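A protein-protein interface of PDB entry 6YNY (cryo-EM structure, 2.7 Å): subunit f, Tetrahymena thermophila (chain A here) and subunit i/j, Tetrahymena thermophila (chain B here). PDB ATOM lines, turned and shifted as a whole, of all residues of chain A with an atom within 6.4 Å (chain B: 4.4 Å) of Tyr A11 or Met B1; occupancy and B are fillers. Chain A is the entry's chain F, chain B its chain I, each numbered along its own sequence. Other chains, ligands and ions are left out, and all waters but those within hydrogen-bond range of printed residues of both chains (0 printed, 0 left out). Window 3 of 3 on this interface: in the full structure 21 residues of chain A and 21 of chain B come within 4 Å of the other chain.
OE1 of Gln B5 lies close to SD of Met B1.
The backbone NH of Gln B5 lies within hydrogen-bond range of the side-chain amide oxygen of Asn B2, at 3.0 Å.
NH2 of Arg B42 lies within hydrogen-bond range of O of Gly B45, at 3.2 Å.
Met B1 touches Tyr A11.
Arg B42 touches Tyr A11.
Leu A12 touches Tyr B44.
CZ3 of Trp A13 touches OH of Tyr B44, at 3.6 Å.
Of the printed residues of chain B, Asp A10 touches Arg B42 and Tyr B44.
Of chain B, only Met B1 (3.9 Å), Gln B5 (3.4 Å), Arg B42 (3.6 Å), Tyr B44 (3.2 Å), Gly B45 (3.1 Å) and Val B46 (3.5 Å) come within 4 Å of Tyr A11.
Printed residues of chain B within 4 Å of Trp A13: Tyr B44.
Met B1 touches one residue of chain A.
The nearest printed residue of chain A that does not touch Arg B42 is Leu A12 (5.8 Å).
Of the 9 printed residues of chain B, 6 touch a printed residue of chain A.
Hydrophobic or aromatic side chains of chain B within 4 Å of the printed part of chain A: Tyr B44.
Among the printed residues, no Asp or Glu carboxylate lies within 4 Å of a Lys or Arg side-chain nitrogen of the other chain.
The backbone carbonyl oxygen (O) of Asp A10 lies within hydrogen-bond range of the backbone NH (N) of Tyr B44, 3.1 Å away.
OH of Tyr A11 sits at hydrogen-bond distance from NE2 of Gln B5 (3.4 Å).
The backbone carbonyl oxygen of Tyr A11 lies close to the backbone NH of Tyr B44, 3.5 Å away.
O of Tyr A11 sits at hydrogen-bond distance from N of Gly B45, 3.1 Å away.
O of Tyr A11 is in hydrogen-bond range of N of Val B46, at 3.5 Å.
OD1 of Asp A10 lies close to O of Arg B42.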
ATOM      1  N   LYS A   6      22.171 -19.915  10.242  1.00  0.00           N
ATOM      2  CA  LYS A   6      22.862 -20.349  11.452  1.00  0.00           C
ATOM      3  C   LYS A   6      22.025 -20.089  12.695  1.00  0.00           C
ATOM      4  O   LYS A   6      21.920 -20.952  13.573  1.00  0.00           O
ATOM      5  CB  LYS A   6      24.213 -19.651  11.569  1.00  0.00           C
ATOM      6  CG  LYS A   6      25.257 -20.160  10.608  1.00  0.00           C
ATOM      7  CD  LYS A   6      26.602 -19.538  10.888  1.00  0.00           C
ATOM      8  CE  LYS A   6      27.671 -20.091   9.972  1.00  0.00           C
ATOM      9  NZ  LYS A   6      27.375 -19.823   8.543  1.00  0.00           N
ATOM     10  N   MET A   7      21.424 -18.904  12.791  1.00  0.00           N
ATOM     11  CA  MET A   7      20.600 -18.594  13.951  1.00  0.00           C
ATOM     12  C   MET A   7      19.394 -19.517  14.030  1.00  0.00           C
ATOM     13  O   MET A   7      18.972 -19.906  15.124  1.00  0.00           O
ATOM     14  CB  MET A   7      20.156 -17.135  13.898  1.00  0.00           C
ATOM     15  CG  MET A   7      21.297 -16.144  14.002  1.00  0.00           C
ATOM     16  SD  MET A   7      22.159 -16.215  15.578  1.00  0.00           S
ATOM     17  CE  MET A   7      20.868 -15.645  16.668  1.00  0.00           C
ATOM     18  N   GLN A   8      18.829 -19.880  12.882  1.00  0.00           N
ATOM     19  CA  GLN A   8      17.642 -20.720  12.877  1.00  0.00           C
ATOM     20  C   GLN A   8      17.998 -22.182  13.118  1.00  0.00           C
ATOM     21  O   GLN A   8      17.334 -22.862  13.905  1.00  0.00           O
ATOM     22  CB  GLN A   8      16.897 -20.556  11.554  1.00  0.00           C
ATOM     23  CG  GLN A   8      15.500 -21.121  11.542  1.00  0.00           C
ATOM     24  CD  GLN A   8      14.586 -20.444  12.537  1.00  0.00           C
ATOM     25  OE1 GLN A   8      14.933 -19.424  13.125  1.00  0.00           O
ATOM     26  NE2 GLN A   8      13.407 -21.008  12.727  1.00  0.00           N
ATOM     27  N   THR A   9      19.042 -22.676  12.452  1.00  0.00           N
ATOM     28  CA  THR A   9      19.403 -24.082  12.589  1.00  0.00           C
ATOM     29  C   THR A   9      19.754 -24.425  14.031  1.00  0.00           C
ATOM     30  O   THR A   9      19.414 -25.507  14.520  1.00  0.00           O
ATOM     31  CB  THR A   9      20.563 -24.420  11.655  1.00  0.00           C
ATOM     32  OG1 THR A   9      21.616 -23.465  11.822  1.00  0.00           O
ATOM     33  CG2 THR A   9      20.099 -24.405  10.218  1.00  0.00           C
ATOM     34  N   ASP A  10      20.441 -23.517  14.726  1.00  0.00           N
ATOM     35  CA  ASP A  10      20.735 -23.735  16.135  1.00  0.00           C
ATOM     36  C   ASP A  10      19.466 -23.720  16.975  1.00  0.00           C
ATOM     37  O   ASP A  10      19.411 -24.362  18.029  1.00  0.00           O
ATOM     38  CB  ASP A  10      21.724 -22.680  16.623  1.00  0.00           C
ATOM     39  CG  ASP A  10      22.019 -22.787  18.102  1.00  0.00           C
ATOM     40  OD1 ASP A  10      21.111 -22.517  18.916  1.00  0.00           O
ATOM     41  OD2 ASP A  10      23.161 -23.147  18.454  1.00  0.00           O
ATOM     42  N   TYR A  11      18.442 -22.998  16.524  1.00  0.00           N
ATOM     43  CA  TYR A  11      17.199 -22.894  17.273  1.00  0.00           C
ATOM     44  C   TYR A  11      16.355 -24.157  17.148  1.00  0.00           C
ATOM     45  O   TYR A  11      15.564 -24.458  18.048  1.00  0.00           O
ATOM     46  CB  TYR A  11      16.423 -21.669  16.785  1.00  0.00           C
ATOM     47  CG  TYR A  11      15.220 -21.280  17.610  1.00  0.00           C
ATOM     48  CD1 TYR A  11      15.364 -20.722  18.868  1.00  0.00           C
ATOM     49  CD2 TYR A  11      13.939 -21.436  17.110  1.00  0.00           C
ATOM     50  CE1 TYR A  11      14.263 -20.353  19.615  1.00  0.00           C
ATOM     51  CE2 TYR A  11      12.838 -21.071  17.846  1.00  0.00           C
ATOM     52  CZ  TYR A  11      13.003 -20.528  19.095  1.00  0.00           C
ATOM     53  OH  TYR A  11      11.895 -20.166  19.825  1.00  0.00           O
ATOM     54  N   LEU A  12      16.510 -24.904  16.056  1.00  0.00           N
ATOM     55  CA  LEU A  12      15.657 -26.056  15.794  1.00  0.00           C
ATOM     56  C   LEU A  12      16.171 -27.341  16.421  1.00  0.00           C
ATOM     57  O   LEU A  12      15.363 -28.197  16.794  1.00  0.00           O
ATOM     58  CB  LEU A  12      15.509 -26.289  14.288  1.00  0.00           C
ATOM     59  CG  LEU A  12      14.435 -25.532  13.500  1.00  0.00           C
ATOM     60  CD1 LEU A  12      13.112 -25.465  14.231  1.00  0.00           C
ATOM     61  CD2 LEU A  12      14.905 -24.161  13.164  1.00  0.00           C
ATOM     62  N   TRP A  13      17.485 -27.514  16.521  1.00  0.00           N
ATOM     63  CA  TRP A  13      18.064 -28.801  16.866  1.00  0.00           C
ATOM     64  C   TRP A  13      19.236 -28.611  17.818  1.00  0.00           C
ATOM     65  O   TRP A  13      19.757 -27.507  17.990  1.00  0.00           O
ATOM     66  CB  TRP A  13      18.494 -29.552  15.601  1.00  0.00           C
ATOM     67  CG  TRP A  13      18.786 -30.993  15.817  1.00  0.00           C
ATOM     68  CD1 TRP A  13      19.918 -31.654  15.467  1.00  0.00           C
ATOM     69  CD2 TRP A  13      17.934 -31.957  16.441  1.00  0.00           C
ATOM     70  NE1 TRP A  13      19.830 -32.972  15.831  1.00  0.00           N
ATOM     71  CE2 TRP A  13      18.619 -33.183  16.432  1.00  0.00           C
ATOM     72  CE3 TRP A  13      16.660 -31.902  17.008  1.00  0.00           C
ATOM     73  CZ2 TRP A  13      18.074 -34.343  16.965  1.00  0.00           C
ATOM     74  CZ3 TRP A  13      16.123 -33.052  17.533  1.00  0.00           C
ATOM     75  CH2 TRP A  13      16.827 -34.256  17.510  1.00  0.00           C
ATOM     76  N   MET B   1      13.512 -16.757  18.197  1.00  0.00           N
ATOM     77  CA  MET B   1      13.451 -15.595  19.126  1.00  0.00           C
ATOM     78  C   MET B   1      12.077 -14.931  19.095  1.00  0.00           C
ATOM     79  O   MET B   1      11.480 -14.773  18.032  1.00  0.00           O
ATOM     80  CB  MET B   1      14.525 -14.579  18.766  1.00  0.00           C
ATOM     81  CG  MET B   1      14.901 -13.681  19.907  1.00  0.00           C
ATOM     82  SD  MET B   1      15.818 -14.572  21.166  1.00  0.00           S
ATOM     83  CE  MET B   1      16.032 -13.278  22.367  1.00  0.00           C
ATOM     84  N   ASN B   2      11.583 -14.538  20.266  1.00  0.00           N
ATOM     85  CA  ASN B   2      10.275 -13.906  20.376  1.00  0.00           C
ATOM     86  C   ASN B   2      10.323 -12.802  21.425  1.00  0.00           C
ATOM     87  O   ASN B   2      11.316 -12.683  22.154  1.00  0.00           O
ATOM     88  CB  ASN B   2       9.196 -14.938  20.719  1.00  0.00           C
ATOM     89  CG  ASN B   2       9.331 -15.495  22.118  1.00  0.00           C
ATOM     90  OD1 ASN B   2       9.297 -14.759  23.102  1.00  0.00           O
ATOM     91  ND2 ASN B   2       9.445 -16.807  22.214  1.00  0.00           N
ATOM     92  N   GLN B   5      11.356 -13.695  25.030  1.00  0.00           N
ATOM     93  CA  GLN B   5      12.776 -13.958  25.224  1.00  0.00           C
ATOM     94  C   GLN B   5      13.569 -12.663  25.310  1.00  0.00           C
ATOM     95  O   GLN B   5      14.536 -12.569  26.073  1.00  0.00           O
ATOM     96  CB  GLN B   5      13.303 -14.830  24.088  1.00  0.00           C
ATOM     97  CG  GLN B   5      12.620 -16.172  23.982  1.00  0.00           C
ATOM     98  CD  GLN B   5      13.125 -16.994  22.820  1.00  0.00           C
ATOM     99  OE1 GLN B   5      14.237 -16.792  22.339  1.00  0.00           O
ATOM    100  NE2 GLN B   5      12.306 -17.924  22.357  1.00  0.00           N
ATOM    101  N   LYS B   6      13.177 -11.653  24.533  1.00  0.00           N
ATOM    102  CA  LYS B   6      13.850 -10.364  24.607  1.00  0.00           C
ATOM    103  C   LYS B   6      13.594  -9.680  25.943  1.00  0.00           C
ATOM    104  O   LYS B   6      14.476  -8.997  26.475  1.00  0.00           O
ATOM    105  CB  LYS B   6      13.394  -9.474  23.457  1.00  0.00           C
ATOM    106  CG  LYS B   6      13.639 -10.070  22.090  1.00  0.00           C
ATOM    107  CD  LYS B   6      13.174  -9.143  20.992  1.00  0.00           C
ATOM    108  CE  LYS B   6      13.360  -9.766  19.628  1.00  0.00           C
ATOM    109  NZ  LYS B   6      14.773 -10.109  19.365  1.00  0.00           N
ATOM    110  N   LEU B   9      15.990 -10.814  28.437  1.00  0.00           N
ATOM    111  CA  LEU B   9      17.344 -10.313  28.235  1.00  0.00           C
ATOM    112  C   LEU B   9      17.569  -8.995  28.962  1.00  0.00           C
ATOM    113  O   LEU B   9      18.583  -8.821  29.648  1.00  0.00           O
ATOM    114  CB  LEU B   9      17.614 -10.155  26.743  1.00  0.00           C
ATOM    115  CG  LEU B   9      17.716 -11.453  25.947  1.00  0.00           C
ATOM    116  CD1 LEU B   9      17.793 -11.161  24.472  1.00  0.00           C
ATOM    117  CD2 LEU B   9      18.921 -12.255  26.380  1.00  0.00           C
ATOM    118  N   ARG B  42      18.659 -19.508  22.346  1.00  0.00           N
ATOM    119  CA  ARG B  42      18.305 -20.819  22.871  1.00  0.00           C
ATOM    120  C   ARG B  42      18.637 -21.911  21.865  1.00  0.00           C
ATOM    121  O   ARG B  42      18.184 -21.871  20.718  1.00  0.00           O
ATOM    122  CB  ARG B  42      16.823 -20.847  23.216  1.00  0.00           C
ATOM    123  CG  ARG B  42      16.437 -19.929  24.342  1.00  0.00           C
ATOM    124  CD  ARG B  42      14.965 -19.613  24.306  1.00  0.00           C
ATOM    125  NE  ARG B  42      14.146 -20.799  24.103  1.00  0.00           N
ATOM    126  CZ  ARG B  42      13.757 -21.617  25.070  1.00  0.00           C
ATOM    127  NH1 ARG B  42      14.113 -21.393  26.322  1.00  0.00           N
ATOM    128  NH2 ARG B  42      13.012 -22.666  24.781  1.00  0.00           N
ATOM    129  N   TYR B  44      17.862 -25.366  20.524  1.00  0.00           N
ATOM    130  CA  TYR B  44      16.650 -26.181  20.503  1.00  0.00           C
ATOM    131  C   TYR B  44      15.528 -25.498  21.279  1.00  0.00           C
ATOM    132  O   TYR B  44      14.793 -26.134  22.034  1.00  0.00           O
ATOM    133  CB  TYR B  44      16.921 -27.581  21.057  1.00  0.00           C
ATOM    134  CG  TYR B  44      15.964 -28.673  20.606  1.00  0.00           C
ATOM    135  CD1 TYR B  44      15.008 -28.449  19.629  1.00  0.00           C
ATOM    136  CD2 TYR B  44      16.020 -29.935  21.172  1.00  0.00           C
ATOM    137  CE1 TYR B  44      14.155 -29.447  19.227  1.00  0.00           C
ATOM    138  CE2 TYR B  44      15.177 -30.935  20.773  1.00  0.00           C
ATOM    139  CZ  TYR B  44      14.242 -30.689  19.805  1.00  0.00           C
ATOM    140  OH  TYR B  44      13.396 -31.698  19.416  1.00  0.00           O
ATOM    141  N   GLY B  45      15.401 -24.190  21.097  1.00  0.00           N
ATOM    142  CA  GLY B  45      14.419 -23.396  21.795  1.00  0.00           C
ATOM    143  C   GLY B  45      13.046 -23.364  21.174  1.00  0.00           C
ATOM    144  O   GLY B  45      12.178 -22.625  21.643  1.00  0.00           O
ATOM    145  N   VAL B  46      12.822 -24.148  20.122  1.00  0.00           N
ATOM    146  CA  VAL B  46      11.512 -24.195  19.499  1.00  0.00           C
ATOM    147  C   VAL B  46      10.489 -24.761  20.477  1.00  0.00           C
ATOM    148  O   VAL B  46      10.814 -25.555  21.368  1.00  0.00           O
ATOM    149  CB  VAL B  46      11.567 -25.027  18.207  1.00  0.00           C
ATOM    150  CG1 VAL B  46      12.036 -26.433  18.500  1.00  0.00           C
ATOM    151  CG2 VAL B  46      10.221 -25.055  17.549  1.00  0.00           C
